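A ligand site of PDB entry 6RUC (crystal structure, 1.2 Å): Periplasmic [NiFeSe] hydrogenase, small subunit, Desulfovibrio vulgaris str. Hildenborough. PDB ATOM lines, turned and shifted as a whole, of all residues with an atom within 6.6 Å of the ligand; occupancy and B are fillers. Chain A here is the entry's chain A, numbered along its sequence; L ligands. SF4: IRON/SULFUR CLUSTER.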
ATOM      1  N   ILE A 207      -8.463  -2.988  21.736  1.00  0.00           N
ATOM      2  CA  ILE A 207      -7.239  -2.933  22.543  1.00  0.00           C
ATOM      3  C   ILE A 207      -7.561  -2.871  24.027  1.00  0.00           C
ATOM      4  O   ILE A 207      -7.078  -3.659  24.833  1.00  0.00           O
ATOM      5  CB  ILE A 207      -6.383  -1.729  22.100  1.00  0.00           C
ATOM      6  CG1 ILE A 207      -5.801  -1.986  20.709  1.00  0.00           C
ATOM      7  CG2 ILE A 207      -5.282  -1.429  23.147  1.00  0.00           C
ATOM      8  CD1 ILE A 207      -4.839  -0.985  20.281  1.00  0.00           C
ATOM      9  N   HIS A 208      -8.387  -1.889  24.409  1.00  0.00           N
ATOM     10  CA  HIS A 208      -8.632  -1.601  25.826  1.00  0.00           C
ATOM     11  C   HIS A 208      -9.273  -2.780  26.545  1.00  0.00           C
ATOM     12  O   HIS A 208      -8.889  -3.124  27.673  1.00  0.00           O
ATOM     13  CB  HIS A 208      -9.519  -0.349  25.890  1.00  0.00           C
ATOM     14  CG  HIS A 208     -10.055  -0.008  27.240  1.00  0.00           C
ATOM     15  ND1 HIS A 208      -9.311   0.679  28.180  1.00  0.00           N
ATOM     16  CD2 HIS A 208     -11.284  -0.182  27.776  1.00  0.00           C
ATOM     17  CE1 HIS A 208     -10.053   0.873  29.254  1.00  0.00           C
ATOM     18  NE2 HIS A 208     -11.253   0.365  29.034  1.00  0.00           N
ATOM     19  N   GLU A 209     -10.258  -3.429  25.926  1.00  0.00           N
ATOM     20  CA  GLU A 209     -10.934  -4.536  26.598  1.00  0.00           C
ATOM     21  C   GLU A 209     -10.023  -5.725  26.828  1.00  0.00           C
ATOM     22  O   GLU A 209     -10.362  -6.591  27.652  1.00  0.00           O
ATOM     23  CB  GLU A 209     -12.184  -4.959  25.821  1.00  0.00           C
ATOM     24  CG  GLU A 209     -13.190  -3.853  25.638  1.00  0.00           C
ATOM     25  CD  GLU A 209     -13.729  -3.308  26.936  1.00  0.00           C
ATOM     26  OE1 GLU A 209     -13.851  -4.063  27.928  1.00  0.00           O
ATOM     27  OE2 GLU A 209     -14.044  -2.100  26.986  1.00  0.00           O
ATOM     28  N   CYS A 211      -6.550  -5.092  27.448  1.00  0.00           N
ATOM     29  CA  CYS A 211      -5.307  -4.458  27.840  1.00  0.00           C
ATOM     30  C   CYS A 211      -4.824  -4.958  29.206  1.00  0.00           C
ATOM     31  O   CYS A 211      -5.632  -5.083  30.127  1.00  0.00           O
ATOM     32  CB  CYS A 211      -5.492  -2.945  27.930  1.00  0.00           C
ATOM     33  SG  CYS A 211      -3.975  -2.060  28.384  1.00  0.00           S
ATOM     34  N   PRO A 212      -3.521  -5.207  29.374  1.00  0.00           N
ATOM     35  CA  PRO A 212      -3.009  -5.600  30.691  1.00  0.00           C
ATOM     36  C   PRO A 212      -3.199  -4.561  31.791  1.00  0.00           C
ATOM     37  O   PRO A 212      -3.114  -4.921  32.968  1.00  0.00           O
ATOM     38  CB  PRO A 212      -1.516  -5.886  30.426  1.00  0.00           C
ATOM     39  CG  PRO A 212      -1.213  -5.174  29.193  1.00  0.00           C
ATOM     40  CD  PRO A 212      -2.462  -5.176  28.361  1.00  0.00           C
ATOM     41  N   TYR A 213      -3.477  -3.300  31.469  1.00  0.00           N
ATOM     42  CA  TYR A 213      -3.657  -2.275  32.487  1.00  0.00           C
ATOM     43  C   TYR A 213      -5.129  -1.978  32.759  1.00  0.00           C
ATOM     44  O   TYR A 213      -5.439  -1.014  33.468  1.00  0.00           O
ATOM     45  CB  TYR A 213      -2.871  -1.006  32.118  1.00  0.00           C
ATOM     46  CG  TYR A 213      -1.463  -1.358  31.706  1.00  0.00           C
ATOM     47  CD1 TYR A 213      -0.548  -1.903  32.620  1.00  0.00           C
ATOM     48  CD2 TYR A 213      -1.054  -1.231  30.391  1.00  0.00           C
ATOM     49  CE1 TYR A 213       0.745  -2.271  32.202  1.00  0.00           C
ATOM     50  CE2 TYR A 213       0.222  -1.585  29.985  1.00  0.00           C
ATOM     51  CZ  TYR A 213       1.108  -2.108  30.892  1.00  0.00           C
ATOM     52  OH  TYR A 213       2.380  -2.469  30.452  1.00  0.00           O
ATOM     53  N   LEU A 214      -6.037  -2.823  32.246  1.00  0.00           N
ATOM     54  CA  LEU A 214      -7.470  -2.575  32.380  1.00  0.00           C
ATOM     55  C   LEU A 214      -7.910  -2.532  33.843  1.00  0.00           C
ATOM     56  O   LEU A 214      -8.805  -1.764  34.199  1.00  0.00           O
ATOM     57  CB  LEU A 214      -8.257  -3.637  31.616  1.00  0.00           C
ATOM     58  CG  LEU A 214      -9.769  -3.452  31.553  1.00  0.00           C
ATOM     59  CD1 LEU A 214     -10.163  -2.118  30.905  1.00  0.00           C
ATOM     60  CD2 LEU A 214     -10.395  -4.604  30.774  1.00  0.00           C
ATOM     61  N   ASP A 215      -7.293  -3.344  34.695  1.00  0.00           N
ATOM     62  CA  ASP A 215      -7.611  -3.310  36.126  1.00  0.00           C
ATOM     63  C   ASP A 215      -7.308  -1.935  36.707  1.00  0.00           C
ATOM     64  O   ASP A 215      -8.089  -1.385  37.502  1.00  0.00           O
ATOM     65  CB  ASP A 215      -6.838  -4.404  36.871  1.00  0.00           C
ATOM     66  CG  ASP A 215      -5.296  -4.310  36.720  1.00  0.00           C
ATOM     67  OD1 ASP A 215      -4.781  -3.896  35.661  1.00  0.00           O
ATOM     68  OD2 ASP A 215      -4.584  -4.695  37.677  1.00  0.00           O
ATOM     69  N   LYS A 216      -6.167  -1.366  36.324  1.00  0.00           N
ATOM     70  CA  LYS A 216      -5.807  -0.030  36.799  1.00  0.00           C
ATOM     71  C   LYS A 216      -6.794   1.014  36.312  1.00  0.00           C
ATOM     72  O   LYS A 216      -7.192   1.901  37.078  1.00  0.00           O
ATOM     73  CB  LYS A 216      -4.379   0.314  36.376  1.00  0.00           C
ATOM     74  CG  LYS A 216      -3.324  -0.648  36.903  1.00  0.00           C
ATOM     75  CD  LYS A 216      -3.304  -0.699  38.437  1.00  0.00           C
ATOM     76  CE  LYS A 216      -2.260  -1.676  38.921  1.00  0.00           C
ATOM     77  NZ  LYS A 216      -2.282  -1.765  40.379  1.00  0.00           N
ATOM     78  N   TYR A 217      -7.191   0.931  35.039  1.00  0.00           N
ATOM     79  CA  TYR A 217      -8.222   1.837  34.519  1.00  0.00           C
ATOM     80  C   TYR A 217      -9.483   1.751  35.368  1.00  0.00           C
ATOM     81  O   TYR A 217     -10.028   2.781  35.816  1.00  0.00           O
ATOM     82  CB  TYR A 217      -8.558   1.451  33.079  1.00  0.00           C
ATOM     83  CG  TYR A 217      -9.689   2.241  32.465  1.00  0.00           C
ATOM     84  CD1 TYR A 217      -9.448   3.430  31.798  1.00  0.00           C
ATOM     85  CD2 TYR A 217     -11.005   1.786  32.534  1.00  0.00           C
ATOM     86  CE1 TYR A 217     -10.471   4.150  31.226  1.00  0.00           C
ATOM     87  CE2 TYR A 217     -12.037   2.506  31.957  1.00  0.00           C
ATOM     88  CZ  TYR A 217     -11.760   3.682  31.306  1.00  0.00           C
ATOM     89  OH  TYR A 217     -12.779   4.406  30.726  1.00  0.00           O
ATOM     90  N   ASP A 218      -9.962   0.544  35.601  1.00  0.00           N
ATOM     91  CA  ASP A 218     -11.210   0.383  36.333  1.00  0.00           C
ATOM     92  C   ASP A 218     -11.079   0.871  37.767  1.00  0.00           C
ATOM     93  O   ASP A 218     -12.071   1.335  38.346  1.00  0.00           O
ATOM     94  CB  ASP A 218     -11.679  -1.078  36.259  1.00  0.00           C
ATOM     95  CG  ASP A 218     -12.231  -1.448  34.874  1.00  0.00           C
ATOM     96  OD1 ASP A 218     -12.684  -0.553  34.138  1.00  0.00           O
ATOM     97  OD2 ASP A 218     -12.215  -2.634  34.521  1.00  0.00           O
ATOM     98  N   MET A 222      -4.118   6.035  37.543  1.00  0.00           N
ATOM     99  CA  MET A 222      -3.623   6.597  36.291  1.00  0.00           C
ATOM    100  C   MET A 222      -2.200   7.096  36.467  1.00  0.00           C
ATOM    101  O   MET A 222      -1.895   7.812  37.429  1.00  0.00           O
ATOM    102  CB  MET A 222      -4.470   7.809  35.876  1.00  0.00           C
ATOM    103  CG  MET A 222      -5.899   7.480  35.626  1.00  0.00           C
ATOM    104  SD  MET A 222      -6.042   6.422  34.176  1.00  0.00           S
ATOM    105  CE  MET A 222      -7.783   6.002  34.282  1.00  0.00           C
ATOM    106  N   GLY A 231       0.514   2.397  36.334  1.00  0.00           N
ATOM    107  CA  GLY A 231      -0.833   2.882  36.130  1.00  0.00           C
ATOM    108  C   GLY A 231      -1.312   2.765  34.691  1.00  0.00           C
ATOM    109  O   GLY A 231      -0.554   2.495  33.755  1.00  0.00           O
ATOM    110  N   CYS A 232      -2.620   2.979  34.525  1.00  0.00           N
ATOM    111  CA  CYS A 232      -3.225   3.096  33.210  1.00  0.00           C
ATOM    112  C   CYS A 232      -2.767   4.396  32.551  1.00  0.00           C
ATOM    113  O   CYS A 232      -2.468   5.390  33.222  1.00  0.00           O
ATOM    114  CB  CYS A 232      -4.745   3.035  33.369  1.00  0.00           C
ATOM    115  SG  CYS A 232      -5.738   3.567  31.928  1.00  0.00           S
ATOM    116  N   ARG A 233      -2.702   4.375  31.217  1.00  0.00           N
ATOM    117  CA  ARG A 233      -2.207   5.470  30.393  1.00  0.00           C
ATOM    118  C   ARG A 233      -3.316   6.400  29.890  1.00  0.00           C
ATOM    119  O   ARG A 233      -3.042   7.302  29.086  1.00  0.00           O
ATOM    120  CB  ARG A 233      -1.431   4.889  29.201  1.00  0.00           C
ATOM    121  CG  ARG A 233      -0.061   4.284  29.521  1.00  0.00           C
ATOM    122  CD  ARG A 233      -0.098   2.987  30.337  1.00  0.00           C
ATOM    123  NE  ARG A 233       1.151   2.253  30.099  1.00  0.00           N
ATOM    124  CZ  ARG A 233       1.767   1.441  30.951  1.00  0.00           C
ATOM    125  NH1 ARG A 233       1.272   1.209  32.173  1.00  0.00           N
ATOM    126  NH2 ARG A 233       2.904   0.877  30.581  1.00  0.00           N
ATOM    127  N   TYR A 234      -4.560   6.204  30.349  1.00  0.00           N
ATOM    128  CA  TYR A 234      -5.693   6.988  29.838  1.00  0.00           C
ATOM    129  C   TYR A 234      -5.477   8.508  29.980  1.00  0.00           C
ATOM    130  O   TYR A 234      -5.735   9.275  29.042  1.00  0.00           O
ATOM    131  CB  TYR A 234      -6.967   6.578  30.563  1.00  0.00           C
ATOM    132  CG  TYR A 234      -8.202   7.268  30.048  1.00  0.00           C
ATOM    133  CD1 TYR A 234      -8.797   6.887  28.855  1.00  0.00           C
ATOM    134  CD2 TYR A 234      -8.782   8.289  30.775  1.00  0.00           C
ATOM    135  CE1 TYR A 234      -9.941   7.521  28.393  1.00  0.00           C
ATOM    136  CE2 TYR A 234      -9.923   8.918  30.326  1.00  0.00           C
ATOM    137  CZ  TYR A 234     -10.496   8.539  29.135  1.00  0.00           C
ATOM    138  OH  TYR A 234     -11.627   9.179  28.712  1.00  0.00           O
ATOM    139  N   ASP A 235      -5.074   8.965  31.160  1.00  0.00           N
ATOM    140  CA  ASP A 235      -4.919  10.406  31.350  1.00  0.00           C
ATOM    141  C   ASP A 235      -3.758  10.989  30.534  1.00  0.00           C
ATOM    142  O   ASP A 235      -3.754  12.195  30.257  1.00  0.00           O
ATOM    143  CB  ASP A 235      -4.663  10.743  32.816  1.00  0.00           C
ATOM    144  CG  ASP A 235      -5.925  10.647  33.685  1.00  0.00           C
ATOM    145  OD1 ASP A 235      -7.028  10.459  33.144  1.00  0.00           O
ATOM    146  OD2 ASP A 235      -5.783  10.782  34.928  1.00  0.00           O
ATOM    147  N   CYS A 238      -4.020   7.809  26.116  1.00  0.00           N
ATOM    148  CA  CYS A 238      -4.201   6.531  25.445  1.00  0.00           C
ATOM    149  C   CYS A 238      -5.571   6.427  24.780  1.00  0.00           C
ATOM    150  O   CYS A 238      -6.609   6.645  25.408  1.00  0.00           O
ATOM    151  CB  CYS A 238      -4.023   5.394  26.444  1.00  0.00           C
ATOM    152  SG  CYS A 238      -4.091   3.752  25.683  1.00  0.00           S
ATOM    153  N   LYS A 239      -5.581   6.041  23.499  1.00  0.00           N
ATOM    154  CA  LYS A 239      -6.795   5.876  22.713  1.00  0.00           C
ATOM    155  C   LYS A 239      -7.205   4.410  22.556  1.00  0.00           C
ATOM    156  O   LYS A 239      -8.071   4.100  21.723  1.00  0.00           O
ATOM    157  CB  LYS A 239      -6.657   6.533  21.353  1.00  0.00           C
ATOM    158  CG  LYS A 239      -6.316   8.024  21.413  1.00  0.00           C
ATOM    159  CD  LYS A 239      -7.278   8.800  22.306  1.00  0.00           C
ATOM    160  CE  LYS A 239      -7.078  10.330  22.217  1.00  0.00           C
ATOM    161  NZ  LYS A 239      -5.681  10.722  22.417  1.00  0.00           N
ATOM    162  N   GLY A 240      -6.617   3.514  23.339  1.00  0.00           N
ATOM    163  CA  GLY A 240      -7.021   2.136  23.371  1.00  0.00           C
ATOM    164  C   GLY A 240      -8.523   1.883  23.401  1.00  0.00           C
ATOM    165  O   GLY A 240      -9.015   0.975  22.721  1.00  0.00           O
ATOM    166  N   PRO A 241      -9.282   2.657  24.183  1.00  0.00           N
ATOM    167  CA  PRO A 241     -10.735   2.397  24.267  1.00  0.00           C
ATOM    168  C   PRO A 241     -11.452   2.480  22.938  1.00  0.00           C
ATOM    169  O   PRO A 241     -12.476   1.810  22.762  1.00  0.00           O
ATOM    170  CB  PRO A 241     -11.217   3.467  25.275  1.00  0.00           C
ATOM    171  CG  PRO A 241     -10.034   3.697  26.147  1.00  0.00           C
ATOM    172  CD  PRO A 241      -8.849   3.618  25.217  1.00  0.00           C
ATOM    173  N   TRP A 258       5.336  -2.566  22.701  1.00  0.00           N
ATOM    174  CA  TRP A 258       4.188  -2.056  21.962  1.00  0.00           C
ATOM    175  C   TRP A 258       3.824  -0.693  22.527  1.00  0.00           C
ATOM    176  O   TRP A 258       4.333  -0.279  23.576  1.00  0.00           O
ATOM    177  CB  TRP A 258       2.980  -2.999  21.983  1.00  0.00           C
ATOM    178  CG  TRP A 258       2.288  -3.233  23.303  1.00  0.00           C
ATOM    179  CD1 TRP A 258       2.842  -3.736  24.446  1.00  0.00           C
ATOM    180  CD2 TRP A 258       0.892  -3.018  23.587  1.00  0.00           C
ATOM    181  NE1 TRP A 258       1.877  -3.845  25.420  1.00  0.00           N
ATOM    182  CE2 TRP A 258       0.671  -3.429  24.921  1.00  0.00           C
ATOM    183  CE3 TRP A 258      -0.200  -2.562  22.838  1.00  0.00           C
ATOM    184  CZ2 TRP A 258      -0.579  -3.357  25.523  1.00  0.00           C
ATOM    185  CZ3 TRP A 258      -1.439  -2.501  23.441  1.00  0.00           C
ATOM    186  CH2 TRP A 258      -1.620  -2.901  24.768  1.00  0.00           C
ATOM    187  N   VAL A 260       1.315   0.860  23.997  1.00  0.00           N
ATOM    188  CA  VAL A 260       0.747   1.106  25.323  1.00  0.00           C
ATOM    189  C   VAL A 260       1.785   0.869  26.409  1.00  0.00           C
ATOM    190  O   VAL A 260       1.848   1.614  27.391  1.00  0.00           O
ATOM    191  CB  VAL A 260      -0.522   0.274  25.532  1.00  0.00           C
ATOM    192  CG1 VAL A 260      -1.034   0.383  26.973  1.00  0.00           C
ATOM    193  CG2 VAL A 260      -1.596   0.714  24.571  1.00  0.00           C
ATOM    194  N   ALA A 263       4.384   3.997  25.826  1.00  0.00           N
ATOM    195  CA  ALA A 263       3.873   5.367  25.846  1.00  0.00           C
ATOM    196  C   ALA A 263       2.346   5.301  25.877  1.00  0.00           C
ATOM    197  O   ALA A 263       1.780   4.924  26.911  1.00  0.00           O
ATOM    198  CB  ALA A 263       4.414   6.172  24.664  1.00  0.00           C
ATOM    199  N   CYS A 265      -1.326   4.417  23.131  1.00  0.00           N
ATOM    200  CA  CYS A 265      -1.909   4.132  21.816  1.00  0.00           C
ATOM    201  C   CYS A 265      -2.471   5.431  21.251  1.00  0.00           C
ATOM    202  O   CYS A 265      -3.121   6.190  21.963  1.00  0.00           O
ATOM    203  CB  CYS A 265      -3.016   3.075  21.942  1.00  0.00           C
ATOM    204  SG  CYS A 265      -3.966   2.698  20.439  1.00  0.00           S
HETATM  205 FE1  SF4 L   1      -5.006   2.469  27.390  1.00  0.00          FE
HETATM  206 FE2  SF4 L   1      -7.288   1.196  28.249  1.00  0.00          FE
HETATM  207 FE3  SF4 L   1      -5.584   2.180  30.101  1.00  0.00          FE
HETATM  208 FE4  SF4 L   1      -4.906   0.015  28.591  1.00  0.00          FE
HETATM  209  S1  SF4 L   1      -6.532   0.110  30.165  1.00  0.00           S
HETATM  210  S2  SF4 L   1      -3.573   1.808  29.108  1.00  0.00           S
HETATM  211  S3  SF4 L   1      -5.902   0.535  26.553  1.00  0.00           S
HETATM  212  S4  SF4 L   1      -6.778   3.416  28.510  1.00  0.00           S
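An iron atom (FE2) of the ligand is bound by a ring nitrogen (ND1) of His 208 (2.1 Å). The side-chain sulfur (SG) of Cys 211 is bound to an iron atom (FE4) of the ligand (2.3 Å). SG of Cys 232 is bound to FE3 of the ligand (2.3 Å). FE1 of the ligand is bound by SG of Cys 238 (2.3 Å). N of Arg 233 lies close to S2 of the ligand (3.4 Å). S1 of the ligand lies close to N of Leu 214 (3.6 Å).
The backbone NH (N) of His 208 lies within hydrogen-bond range of the backbone carbonyl oxygen (O) of Gly 240, at 3.4 Å. The side-chain sulfur of Cys 211 lies close to the backbone NH of Tyr 213, at 3.4 Å. The side-chain sulfur (SG) of Cys 232 sits close to the backbone NH (N) of Tyr 234 (3.3 Å). SG of Cys 232 lies close to SD of Met 222 (3.6 Å). O of Arg 233 lies within hydrogen-bond range of N of Cys 238 (3.2 Å). The backbone NH (N) of Gly 240 sits close to the side-chain sulfur (SG) of Cys 238, at 3.5 Å. NE of Arg 233 lies within hydrogen-bond range of O of Val 260. The side-chain hydroxyl (OH) of Tyr 213 sits at hydrogen-bond distance from the guanidinium group (NH2) of Arg 233 (3.4 Å).
O of Tyr 213 sits close to S1 of the ligand (3.7 Å). CG2 of Ile 207 touches S3 of the ligand, 3.98 Å away. Tyr 217 touches the ligand (CB to S1, 3.8 Å). CB of Tyr 234 touches S4 of the ligand (3.8 Å). CA of Gly 240 touches S3 of the ligand, 3.7 Å away. Pro 241 touches the ligand. Val 260 touches the ligand. Hydrophobic or aromatic side chains within 4 Å of the ligand: Ile 207, His 208, Tyr 217, Tyr 234, Pro 241 and Val 260. Within 4 Å of the ligand: Ile 207, His 208, Cys 211, Tyr 213, Leu 214, Tyr 217, Cys 232, Arg 233, Tyr 234, Cys 238, Gly 240, Pro 241 and Val 260.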
